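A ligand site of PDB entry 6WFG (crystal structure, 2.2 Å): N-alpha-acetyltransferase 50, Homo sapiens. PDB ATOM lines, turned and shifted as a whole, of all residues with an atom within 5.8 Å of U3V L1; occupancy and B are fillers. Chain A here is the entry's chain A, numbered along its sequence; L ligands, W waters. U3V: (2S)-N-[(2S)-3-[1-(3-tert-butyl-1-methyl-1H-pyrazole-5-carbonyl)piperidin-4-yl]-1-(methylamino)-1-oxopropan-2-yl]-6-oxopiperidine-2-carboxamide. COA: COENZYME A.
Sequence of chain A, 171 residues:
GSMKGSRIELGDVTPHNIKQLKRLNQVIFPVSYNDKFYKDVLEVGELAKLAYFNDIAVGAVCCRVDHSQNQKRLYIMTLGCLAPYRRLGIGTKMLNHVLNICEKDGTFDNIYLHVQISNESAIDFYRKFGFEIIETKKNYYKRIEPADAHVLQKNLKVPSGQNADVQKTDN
OH of Tyr 141 sits at hydrogen-bond distance from O2 of U3V L1 (2.6 Å). The side-chain hydroxyl (OH) of Tyr 33 sits at hydrogen-bond distance from an oxygen (O1) of U3V L1 (2.7 Å). The backbone carbonyl oxygen (O) of His 114 is in hydrogen-bond range of a nitrogen (N4) of U3V L1, at 2.8 Å. The backbone carbonyl oxygen of Met 77 lies within hydrogen-bond range of a nitrogen (N2) of U3V L1, 2.9 Å away. The guanidinium group of Arg 64 lies within hydrogen-bond range of an oxygen (O4) of U3V L1, at 2.9 Å. An oxygen (O3) of U3V L1 lies within hydrogen-bond range of the backbone NH of Gln 116 (3.0 Å). The side-chain hydroxyl of Tyr 140 sits at hydrogen-bond distance from a nitrogen (N3) of U3V L1 (3.2 Å). ND2 of Asn 119 lies within hydrogen-bond range of O5P of COA L2, 2.9 Å away.
The backbone NH of Gln 116 sits at hydrogen-bond distance from the side-chain hydroxyl of Tyr 141 (3.5 Å). The side-chain hydroxyl (OH) of Tyr 140 is in hydrogen-bond range of a ring nitrogen (ND1) of His 114 (3.2 Å). A ring nitrogen (ND1) of His 114 is in hydrogen-bond range of the side-chain hydroxyl of Tyr 75, at 2.8 Å. O of Arg 64 lies within hydrogen-bond range of N of Tyr 75, 3.0 Å away. The side-chain carboxylate of Asp 40 is in salt-bridge range of the guanidinium group of Arg 64, 3.3 Å away. The side-chain hydroxyl (OH) of Tyr 75 sits at hydrogen-bond distance from the side-chain hydroxyl (OH) of Tyr 140, at 3.3 Å. The side-chain carboxylate (OD2) of Asp 66 is in hydrogen-bond range of the side-chain hydroxyl (OH) of Tyr 112, at 2.7 Å. The backbone carbonyl oxygen (O) of Tyr 112 lies within hydrogen-bond range of the backbone NH (N) of Ile 76 (3.0 Å).
Residues that only touch U3V L1: Val 31 (3.5 Å), Tyr 112 (3.5 Å), Asp 66 (3.6 Å), Tyr 75 (3.6 Å), Val 115 (3.7 Å), Pro 30 (3.9 Å) and Phe 29 (3.998 Å). Within 4 Å of U3V L1: Phe 29, Pro 30, Val 31, Tyr 33, Arg 64, Asp 66, Tyr 75, Met 77, Tyr 112, His 114, Val 115, Gln 116, Tyr 140 and Tyr 141.
Water W1 lies within hydrogen-bond range of O of Ile 76 (2.7 Å), N of His 114 (2.8 Å), OH of Tyr 75 (3.1 Å) and N2 of U3V L1 (3.3 Å).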
ATOM      1  N   PHE A  29      -0.231  13.782 -15.944  1.00  0.00           N
ATOM      2  CA  PHE A  29      -0.371  12.560 -16.704  1.00  0.00           C
ATOM      3  C   PHE A  29      -0.503  12.748 -18.225  1.00  0.00           C
ATOM      4  O   PHE A  29      -1.088  13.733 -18.663  1.00  0.00           O
ATOM      5  CB  PHE A  29      -1.545  11.719 -16.145  1.00  0.00           C
ATOM      6  CG  PHE A  29      -1.311  11.419 -14.679  1.00  0.00           C
ATOM      7  CD1 PHE A  29      -0.302  10.549 -14.289  1.00  0.00           C
ATOM      8  CD2 PHE A  29      -2.028  12.096 -13.689  1.00  0.00           C
ATOM      9  CE1 PHE A  29      -0.057  10.306 -12.931  1.00  0.00           C
ATOM     10  CE2 PHE A  29      -1.768  11.867 -12.338  1.00  0.00           C
ATOM     11  CZ  PHE A  29      -0.801  10.963 -11.969  1.00  0.00           C
ATOM     12  N   PRO A  30       0.025  11.765 -19.031  1.00  0.00           N
ATOM     13  CA  PRO A  30      -0.058  11.862 -20.508  1.00  0.00           C
ATOM     14  C   PRO A  30      -1.401  11.375 -21.092  1.00  0.00           C
ATOM     15  O   PRO A  30      -1.559  11.337 -22.311  1.00  0.00           O
ATOM     16  CB  PRO A  30       1.073  10.936 -20.957  1.00  0.00           C
ATOM     17  CG  PRO A  30       1.066   9.853 -19.929  1.00  0.00           C
ATOM     18  CD  PRO A  30       0.726  10.522 -18.622  1.00  0.00           C
ATOM     19  N   VAL A  31      -2.327  10.954 -20.217  1.00  0.00           N
ATOM     20  CA  VAL A  31      -3.658  10.437 -20.561  1.00  0.00           C
ATOM     21  C   VAL A  31      -4.701  11.459 -20.053  1.00  0.00           C
ATOM     22  O   VAL A  31      -4.559  11.965 -18.940  1.00  0.00           O
ATOM     23  CB  VAL A  31      -3.873   9.047 -19.880  1.00  0.00           C
ATOM     24  CG1 VAL A  31      -5.311   8.553 -20.038  1.00  0.00           C
ATOM     25  CG2 VAL A  31      -2.884   7.999 -20.391  1.00  0.00           C
ATOM     26  N   TYR A  33      -8.524  12.161 -18.802  1.00  0.00           N
ATOM     27  CA  TYR A  33      -9.596  11.367 -18.222  1.00  0.00           C
ATOM     28  C   TYR A  33     -10.964  12.010 -18.432  1.00  0.00           C
ATOM     29  O   TYR A  33     -11.092  13.242 -18.396  1.00  0.00           O
ATOM     30  CB  TYR A  33      -9.311  11.020 -16.742  1.00  0.00           C
ATOM     31  CG  TYR A  33      -8.048  10.213 -16.585  1.00  0.00           C
ATOM     32  CD1 TYR A  33      -8.009   8.879 -16.941  1.00  0.00           C
ATOM     33  CD2 TYR A  33      -6.871  10.818 -16.153  1.00  0.00           C
ATOM     34  CE1 TYR A  33      -6.823   8.143 -16.855  1.00  0.00           C
ATOM     35  CE2 TYR A  33      -5.679  10.093 -16.073  1.00  0.00           C
ATOM     36  CZ  TYR A  33      -5.667   8.752 -16.405  1.00  0.00           C
ATOM     37  OH  TYR A  33      -4.504   8.049 -16.332  1.00  0.00           O
ATOM     38  N   LYS A  36     -16.633  10.580 -16.391  1.00  0.00           N
ATOM     39  CA  LYS A  36     -16.997   9.422 -15.572  1.00  0.00           C
ATOM     40  C   LYS A  36     -15.909   9.114 -14.515  1.00  0.00           C
ATOM     41  O   LYS A  36     -16.248   8.671 -13.416  1.00  0.00           O
ATOM     42  CB  LYS A  36     -17.269   8.183 -16.438  1.00  0.00           C
ATOM     43  CG  LYS A  36     -18.023   7.070 -15.696  1.00  0.00           C
ATOM     44  CD  LYS A  36     -17.483   5.690 -16.043  1.00  0.00           C
ATOM     45  CE  LYS A  36     -18.175   4.589 -15.288  1.00  0.00           C
ATOM     46  NZ  LYS A  36     -17.808   3.248 -15.820  1.00  0.00           N
ATOM     47  N   PHE A  37     -14.609   9.300 -14.876  1.00  0.00           N
ATOM     48  CA  PHE A  37     -13.480   9.070 -13.972  1.00  0.00           C
ATOM     49  C   PHE A  37     -13.613   9.997 -12.744  1.00  0.00           C
ATOM     50  O   PHE A  37     -13.545   9.509 -11.614  1.00  0.00           O
ATOM     51  CB  PHE A  37     -12.132   9.315 -14.715  1.00  0.00           C
ATOM     52  CG  PHE A  37     -10.882   9.322 -13.865  1.00  0.00           C
ATOM     53  CD1 PHE A  37     -10.172   8.150 -13.635  1.00  0.00           C
ATOM     54  CD2 PHE A  37     -10.395  10.506 -13.317  1.00  0.00           C
ATOM     55  CE1 PHE A  37      -8.990   8.173 -12.866  1.00  0.00           C
ATOM     56  CE2 PHE A  37      -9.230  10.520 -12.533  1.00  0.00           C
ATOM     57  CZ  PHE A  37      -8.530   9.346 -12.315  1.00  0.00           C
ATOM     58  N   ASP A  40     -16.670   9.060 -10.619  1.00  0.00           N
ATOM     59  CA  ASP A  40     -16.300   7.846  -9.858  1.00  0.00           C
ATOM     60  C   ASP A  40     -15.402   8.246  -8.669  1.00  0.00           C
ATOM     61  O   ASP A  40     -15.561   7.699  -7.570  1.00  0.00           O
ATOM     62  CB  ASP A  40     -15.494   6.873 -10.748  1.00  0.00           C
ATOM     63  CG  ASP A  40     -16.281   5.986 -11.682  1.00  0.00           C
ATOM     64  OD1 ASP A  40     -17.498   5.776 -11.439  1.00  0.00           O
ATOM     65  OD2 ASP A  40     -15.670   5.405 -12.619  1.00  0.00           O
ATOM     66  N   ARG A  64      -9.554   2.601  -7.240  1.00  0.00           N
ATOM     67  CA  ARG A  64     -10.848   1.938  -7.337  1.00  0.00           C
ATOM     68  C   ARG A  64     -10.664   0.514  -6.875  1.00  0.00           C
ATOM     69  O   ARG A  64      -9.558  -0.035  -7.009  1.00  0.00           O
ATOM     70  CB  ARG A  64     -11.470   2.024  -8.769  1.00  0.00           C
ATOM     71  CG  ARG A  64     -10.891   1.043  -9.821  1.00  0.00           C
ATOM     72  CD  ARG A  64     -11.472   1.198 -11.219  1.00  0.00           C
ATOM     73  NE  ARG A  64     -12.935   1.088 -11.248  1.00  0.00           N
ATOM     74  CZ  ARG A  64     -13.750   2.067 -11.644  1.00  0.00           C
ATOM     75  NH1 ARG A  64     -13.248   3.215 -12.073  1.00  0.00           N
ATOM     76  NH2 ARG A  64     -15.063   1.880 -11.636  1.00  0.00           N
ATOM     77  N   VAL A  65     -11.726  -0.086  -6.326  1.00  0.00           N
ATOM     78  CA  VAL A  65     -11.717  -1.481  -5.898  1.00  0.00           C
ATOM     79  C   VAL A  65     -12.042  -2.281  -7.158  1.00  0.00           C
ATOM     80  O   VAL A  65     -12.840  -1.857  -7.982  1.00  0.00           O
ATOM     81  CB  VAL A  65     -12.728  -1.777  -4.745  1.00  0.00           C
ATOM     82  CG1 VAL A  65     -12.607  -3.227  -4.263  1.00  0.00           C
ATOM     83  CG2 VAL A  65     -12.537  -0.813  -3.576  1.00  0.00           C
ATOM     84  N   ASP A  66     -11.363  -3.413  -7.322  1.00  0.00           N
ATOM     85  CA  ASP A  66     -11.551  -4.316  -8.446  1.00  0.00           C
ATOM     86  C   ASP A  66     -11.724  -5.755  -7.968  1.00  0.00           C
ATOM     87  O   ASP A  66     -10.996  -6.209  -7.086  1.00  0.00           O
ATOM     88  CB  ASP A  66     -10.394  -4.199  -9.447  1.00  0.00           C
ATOM     89  CG  ASP A  66     -10.521  -5.114 -10.661  1.00  0.00           C
ATOM     90  OD1 ASP A  66     -11.596  -5.082 -11.329  1.00  0.00           O
ATOM     91  OD2 ASP A  66      -9.558  -5.840 -10.966  1.00  0.00           O
ATOM     92  N   TYR A  75      -6.792  -1.139  -7.224  1.00  0.00           N
ATOM     93  CA  TYR A  75      -6.168  -0.661  -8.449  1.00  0.00           C
ATOM     94  C   TYR A  75      -5.904   0.829  -8.354  1.00  0.00           C
ATOM     95  O   TYR A  75      -6.844   1.604  -8.176  1.00  0.00           O
ATOM     96  CB  TYR A  75      -7.018  -0.977  -9.698  1.00  0.00           C
ATOM     97  CG  TYR A  75      -6.434  -0.472 -11.006  1.00  0.00           C
ATOM     98  CD1 TYR A  75      -5.425  -1.184 -11.663  1.00  0.00           C
ATOM     99  CD2 TYR A  75      -6.899   0.700 -11.585  1.00  0.00           C
ATOM    100  CE1 TYR A  75      -4.915  -0.745 -12.891  1.00  0.00           C
ATOM    101  CE2 TYR A  75      -6.340   1.187 -12.777  1.00  0.00           C
ATOM    102  CZ  TYR A  75      -5.375   0.447 -13.446  1.00  0.00           C
ATOM    103  OH  TYR A  75      -4.837   0.908 -14.624  1.00  0.00           O
ATOM    104  N   ILE A  76      -4.634   1.236  -8.503  1.00  0.00           N
ATOM    105  CA  ILE A  76      -4.284   2.648  -8.477  1.00  0.00           C
ATOM    106  C   ILE A  76      -4.392   3.168  -9.900  1.00  0.00           C
ATOM    107  O   ILE A  76      -3.655   2.721 -10.785  1.00  0.00           O
ATOM    108  CB  ILE A  76      -2.861   2.895  -7.892  1.00  0.00           C
ATOM    109  CG1 ILE A  76      -2.755   2.387  -6.453  1.00  0.00           C
ATOM    110  CG2 ILE A  76      -2.446   4.388  -7.994  1.00  0.00           C
ATOM    111  CD1 ILE A  76      -1.320   2.329  -5.931  1.00  0.00           C
ATOM    112  N   MET A  77      -5.307   4.109 -10.141  1.00  0.00           N
ATOM    113  CA  MET A  77      -5.509   4.641 -11.490  1.00  0.00           C
ATOM    114  C   MET A  77      -4.499   5.733 -11.768  1.00  0.00           C
ATOM    115  O   MET A  77      -3.910   5.772 -12.852  1.00  0.00           O
ATOM    116  CB  MET A  77      -6.946   5.187 -11.682  1.00  0.00           C
ATOM    117  CG  MET A  77      -8.046   4.151 -11.454  1.00  0.00           C
ATOM    118  SD  MET A  77      -9.746   4.847 -11.568  1.00  0.00           S
ATOM    119  CE  MET A  77      -9.813   5.817 -10.033  1.00  0.00           C
ATOM    120  N   THR A  78      -4.339   6.672 -10.794  1.00  0.00           N
ATOM    121  CA  THR A  78      -3.415   7.802 -10.929  1.00  0.00           C
ATOM    122  C   THR A  78      -2.773   8.094  -9.587  1.00  0.00           C
ATOM    123  O   THR A  78      -3.419   8.057  -8.537  1.00  0.00           O
ATOM    124  CB  THR A  78      -4.123   9.082 -11.483  1.00  0.00           C
ATOM    125  OG1 THR A  78      -5.240   9.409 -10.673  1.00  0.00           O
ATOM    126  CG2 THR A  78      -4.573   8.969 -12.915  1.00  0.00           C
ATOM    127  N   TYR A 112      -2.490  -3.268  -7.532  1.00  0.00           N
ATOM    128  CA  TYR A 112      -1.860  -3.223  -8.832  1.00  0.00           C
ATOM    129  C   TYR A 112      -2.145  -1.912  -9.548  1.00  0.00           C
ATOM    130  O   TYR A 112      -2.962  -1.131  -9.077  1.00  0.00           O
ATOM    131  CB  TYR A 112      -2.198  -4.478  -9.661  1.00  0.00           C
ATOM    132  CG  TYR A 112      -3.577  -4.510 -10.284  1.00  0.00           C
ATOM    133  CD1 TYR A 112      -4.721  -4.602  -9.491  1.00  0.00           C
ATOM    134  CD2 TYR A 112      -3.738  -4.523 -11.665  1.00  0.00           C
ATOM    135  CE1 TYR A 112      -5.996  -4.638 -10.059  1.00  0.00           C
ATOM    136  CE2 TYR A 112      -4.999  -4.599 -12.241  1.00  0.00           C
ATOM    137  CZ  TYR A 112      -6.127  -4.673 -11.434  1.00  0.00           C
ATOM    138  OH  TYR A 112      -7.351  -4.744 -12.044  1.00  0.00           O
ATOM    139  N   HIS A 114      -0.896   0.287 -13.688  1.00  0.00           N
ATOM    140  CA  HIS A 114      -0.200   0.275 -14.963  1.00  0.00           C
ATOM    141  C   HIS A 114       0.834   1.373 -14.976  1.00  0.00           C
ATOM    142  O   HIS A 114       0.576   2.491 -14.510  1.00  0.00           O
ATOM    143  CB  HIS A 114      -1.186   0.428 -16.133  1.00  0.00           C
ATOM    144  CG  HIS A 114      -1.985  -0.795 -16.400  1.00  0.00           C
ATOM    145  ND1 HIS A 114      -3.208  -1.008 -15.780  1.00  0.00           N
ATOM    146  CD2 HIS A 114      -1.734  -1.822 -17.242  1.00  0.00           C
ATOM    147  CE1 HIS A 114      -3.653  -2.170 -16.252  1.00  0.00           C
ATOM    148  NE2 HIS A 114      -2.782  -2.712 -17.115  1.00  0.00           N
ATOM    149  N   VAL A 115       2.032   1.055 -15.478  1.00  0.00           N
ATOM    150  CA  VAL A 115       3.109   2.012 -15.585  1.00  0.00           C
ATOM    151  C   VAL A 115       3.645   1.909 -16.994  1.00  0.00           C
ATOM    152  O   VAL A 115       4.232   0.885 -17.351  1.00  0.00           O
ATOM    153  CB  VAL A 115       4.244   1.810 -14.518  1.00  0.00           C
ATOM    154  CG1 VAL A 115       5.428   2.760 -14.772  1.00  0.00           C
ATOM    155  CG2 VAL A 115       3.731   2.002 -13.091  1.00  0.00           C
ATOM    156  N   GLN A 116       3.471   2.992 -17.784  1.00  0.00           N
ATOM    157  CA  GLN A 116       4.018   3.127 -19.144  1.00  0.00           C
ATOM    158  C   GLN A 116       5.526   2.765 -19.050  1.00  0.00           C
ATOM    159  O   GLN A 116       6.203   3.253 -18.146  1.00  0.00           O
ATOM    160  CB  GLN A 116       3.820   4.581 -19.627  1.00  0.00           C
ATOM    161  CG  GLN A 116       4.234   4.823 -21.065  1.00  0.00           C
ATOM    162  CD  GLN A 116       3.936   6.228 -21.555  1.00  0.00           C
ATOM    163  OE1 GLN A 116       3.967   7.222 -20.806  1.00  0.00           O
ATOM    164  NE2 GLN A 116       3.728   6.363 -22.848  1.00  0.00           N
ATOM    165  N   ASN A 119       8.510   5.136 -18.242  1.00  0.00           N
ATOM    166  CA  ASN A 119       8.446   5.808 -16.956  1.00  0.00           C
ATOM    167  C   ASN A 119       9.286   5.071 -15.919  1.00  0.00           C
ATOM    168  O   ASN A 119       8.783   4.350 -15.047  1.00  0.00           O
ATOM    169  CB  ASN A 119       6.995   6.011 -16.526  1.00  0.00           C
ATOM    170  CG  ASN A 119       6.838   7.072 -15.462  1.00  0.00           C
ATOM    171  OD1 ASN A 119       7.816   7.492 -14.818  1.00  0.00           O
ATOM    172  ND2 ASN A 119       5.590   7.435 -15.191  1.00  0.00           N
ATOM    173  N   TYR A 140      -1.109  -1.105 -24.495  1.00  0.00           N
ATOM    174  CA  TYR A 140      -2.075  -0.750 -23.451  1.00  0.00           C
ATOM    175  C   TYR A 140      -2.658   0.636 -23.755  1.00  0.00           C
ATOM    176  O   TYR A 140      -3.862   0.820 -23.612  1.00  0.00           O
ATOM    177  CB  TYR A 140      -1.416  -0.775 -22.066  1.00  0.00           C
ATOM    178  CG  TYR A 140      -2.353  -0.394 -20.950  1.00  0.00           C
ATOM    179  CD1 TYR A 140      -3.355  -1.268 -20.524  1.00  0.00           C
ATOM    180  CD2 TYR A 140      -2.251   0.840 -20.312  1.00  0.00           C
ATOM    181  CE1 TYR A 140      -4.223  -0.921 -19.496  1.00  0.00           C
ATOM    182  CE2 TYR A 140      -3.108   1.189 -19.271  1.00  0.00           C
ATOM    183  CZ  TYR A 140      -4.089   0.311 -18.864  1.00  0.00           C
ATOM    184  OH  TYR A 140      -4.952   0.666 -17.864  1.00  0.00           O
ATOM    185  N   TYR A 141      -1.826   1.598 -24.155  1.00  0.00           N
ATOM    186  CA  TYR A 141      -2.252   2.960 -24.480  1.00  0.00           C
ATOM    187  C   TYR A 141      -2.569   3.105 -25.965  1.00  0.00           C
ATOM    188  O   TYR A 141      -1.983   2.417 -26.798  1.00  0.00           O
ATOM    189  CB  TYR A 141      -1.233   3.991 -24.016  1.00  0.00           C
ATOM    190  CG  TYR A 141      -0.870   3.890 -22.553  1.00  0.00           C
ATOM    191  CD1 TYR A 141      -1.746   4.360 -21.570  1.00  0.00           C
ATOM    192  CD2 TYR A 141       0.339   3.348 -22.144  1.00  0.00           C
ATOM    193  CE1 TYR A 141      -1.419   4.269 -20.216  1.00  0.00           C
ATOM    194  CE2 TYR A 141       0.676   3.255 -20.799  1.00  0.00           C
ATOM    195  CZ  TYR A 141      -0.215   3.707 -19.831  1.00  0.00           C
ATOM    196  OH  TYR A 141       0.120   3.586 -18.504  1.00  0.00           O
HETATM  197  C19 U3V L   1      -9.803   0.469 -14.435  1.00  0.00           C
HETATM  198  C17 U3V L   1     -10.827   1.286 -14.853  1.00  0.00           C
HETATM  199  C18 U3V L   1     -10.395  -0.815 -14.245  1.00  0.00           C
HETATM  200  C12 U3V L   1       0.939   5.754 -16.357  1.00  0.00           C
HETATM  201  C16 U3V L   1     -10.847   2.683 -15.162  1.00  0.00           C
HETATM  202  C10 U3V L   1      -2.314   4.589 -16.033  1.00  0.00           C
HETATM  203  C8  U3V L   1      -4.766   4.723 -17.666  1.00  0.00           C
HETATM  204  C13 U3V L   1       0.491   7.150 -16.659  1.00  0.00           C
HETATM  205  C14 U3V L   1      -1.008   7.338 -16.564  1.00  0.00           C
HETATM  206  C15 U3V L   1      -1.500   6.788 -15.248  1.00  0.00           C
HETATM  207  C3  U3V L   1      -8.388   4.984 -15.500  1.00  0.00           C
HETATM  208  C4  U3V L   1      -7.587   2.762 -16.206  1.00  0.00           C
HETATM  209  C1  U3V L   1      -9.730   4.657 -16.117  1.00  0.00           C
HETATM  210  C2  U3V L   1      -8.946   2.507 -16.823  1.00  0.00           C
HETATM  211  C11 U3V L   1      -1.270   5.307 -15.201  1.00  0.00           C
HETATM  212  C5  U3V L   1      -7.287   4.241 -16.220  1.00  0.00           C
HETATM  213  C21 U3V L   1      -9.741  -1.984 -12.261  1.00  0.00           C
HETATM  214  C22 U3V L   1      -8.277  -2.106 -14.229  1.00  0.00           C
HETATM  215  C23 U3V L   1     -10.420  -3.308 -14.220  1.00  0.00           C
HETATM  216  C24 U3V L   1     -13.282   0.876 -15.208  1.00  0.00           C
HETATM  217  C9  U3V L   1      -5.185   4.237 -20.006  1.00  0.00           C
HETATM  218  C6  U3V L   1      -5.987   4.537 -15.493  1.00  0.00           C
HETATM  219  C7  U3V L   1      -4.741   4.133 -16.269  1.00  0.00           C
HETATM  220  C20 U3V L   1      -9.728  -2.038 -13.770  1.00  0.00           C
HETATM  221  N6  U3V L   1     -11.707  -0.782 -14.478  1.00  0.00           N
HETATM  222  N5  U3V L   1     -11.937   0.470 -14.857  1.00  0.00           N
HETATM  223  N4  U3V L   1       0.040   4.916 -15.710  1.00  0.00           N
HETATM  224  N1  U3V L   1      -9.983   3.225 -16.103  1.00  0.00           N
HETATM  225  N2  U3V L   1      -3.598   4.648 -15.542  1.00  0.00           N
HETATM  226  N3  U3V L   1      -5.046   3.789 -18.649  1.00  0.00           N
HETATM  227  O3  U3V L   1       2.077   5.415 -16.673  1.00  0.00           O
HETATM  228  O4  U3V L   1     -11.636   3.376 -14.520  1.00  0.00           O
HETATM  229  O2  U3V L   1      -2.050   4.019 -17.066  1.00  0.00           O
HETATM  230  O1  U3V L   1      -4.580   5.904 -17.910  1.00  0.00           O
HETATM  231  N1A COA L   2      14.882   8.216  -9.729  1.00  0.00           N
HETATM  232  C2A COA L   2      15.186   7.233  -8.864  1.00  0.00           C
HETATM  233  N3A COA L   2      14.478   6.820  -7.805  1.00  0.00           N
HETATM  234  C4A COA L   2      13.340   7.512  -7.673  1.00  0.00           C
HETATM  235  C5A COA L   2      12.922   8.553  -8.497  1.00  0.00           C
HETATM  236  C6A COA L   2      13.744   8.890  -9.550  1.00  0.00           C
HETATM  237  N6A COA L   2      13.405   9.938 -10.415  1.00  0.00           N
HETATM  238  N7A COA L   2      11.714   9.050  -8.067  1.00  0.00           N
HETATM  239  C8A COA L   2      11.412   8.331  -7.009  1.00  0.00           C
HETATM  240  N9A COA L   2      12.356   7.377  -6.731  1.00  0.00           N
HETATM  241  C1B COA L   2      12.357   6.505  -5.563  1.00  0.00           C
HETATM  242  C2B COA L   2      13.458   6.883  -4.582  1.00  0.00           C
HETATM  243  O2B COA L   2      14.028   5.769  -3.916  1.00  0.00           O
HETATM  244  C3B COA L   2      12.732   7.803  -3.633  1.00  0.00           C
HETATM  245  O3B COA L   2      13.377   7.868  -2.369  1.00  0.00           O
HETATM  246  P3B COA L   2      14.384   9.148  -2.169  1.00  0.00           P
HETATM  247  O7A COA L   2      14.504   9.190  -0.668  1.00  0.00           O
HETATM  248  O8A COA L   2      15.653   8.757  -2.889  1.00  0.00           O
HETATM  249  O9A COA L   2      13.690  10.344  -2.810  1.00  0.00           O
HETATM  250  C4B COA L   2      11.393   7.142  -3.520  1.00  0.00           C
HETATM  251  O4B COA L   2      11.123   6.664  -4.840  1.00  0.00           O
HETATM  252  C5B COA L   2      10.311   8.074  -2.984  1.00  0.00           C
HETATM  253  O5B COA L   2      10.170   9.282  -3.731  1.00  0.00           O
HETATM  254  P1A COA L   2       9.026  10.352  -3.295  1.00  0.00           P
HETATM  255  O1A COA L   2       9.671  11.689  -3.065  1.00  0.00           O
HETATM  256  O2A COA L   2       8.081   9.826  -2.245  1.00  0.00           O
HETATM  257  O3A COA L   2       8.221  10.331  -4.708  1.00  0.00           O
HETATM  258  P2A COA L   2       7.673  11.542  -5.652  1.00  0.00           P
HETATM  259  O4A COA L   2       6.843  12.458  -4.788  1.00  0.00           O
HETATM  260  O5A COA L   2       8.834  12.100  -6.448  1.00  0.00           O
HETATM  261  O6A COA L   2       6.634  10.752  -6.604  1.00  0.00           O
HETATM  262  CBP COA L   2       6.182   9.564  -8.679  1.00  0.00           C
HETATM  263  CCP COA L   2       6.978   9.582  -7.374  1.00  0.00           C
HETATM  264  CDP COA L   2       6.566   8.338  -9.478  1.00  0.00           C
HETATM  265  CEP COA L   2       4.719   9.381  -8.321  1.00  0.00           C
HETATM  266  CAP COA L   2       6.463  10.881  -9.410  1.00  0.00           C
HETATM  267  OAP COA L   2       7.694  10.899 -10.141  1.00  0.00           O
HETATM  268  C9P COA L   2       5.402  11.374 -10.356  1.00  0.00           C
HETATM  269  O9P COA L   2       4.534  12.150  -9.986  1.00  0.00           O
HETATM  270  N8P COA L   2       5.559  10.886 -11.628  1.00  0.00           N
HETATM  271  C7P COA L   2       4.688  11.234 -12.728  1.00  0.00           C
HETATM  272  C6P COA L   2       3.389  10.505 -12.588  1.00  0.00           C
HETATM  273  C5P COA L   2       3.404   9.279 -13.431  1.00  0.00           C
HETATM  274  O5P COA L   2       3.522   9.363 -14.652  1.00  0.00           O
HETATM  275  N4P COA L   2       3.245   8.130 -12.672  1.00  0.00           N
HETATM  276  C3P COA L   2       2.438   7.016 -13.145  1.00  0.00           C
HETATM  277  C2P COA L   2       2.049   6.056 -12.039  1.00  0.00           C
HETATM  278  S1P COA L   2       0.239   6.131 -11.819  1.00  0.00           S
HETATM  279  O   HOH W   1      -2.559   2.501 -13.277  1.00  0.00           O
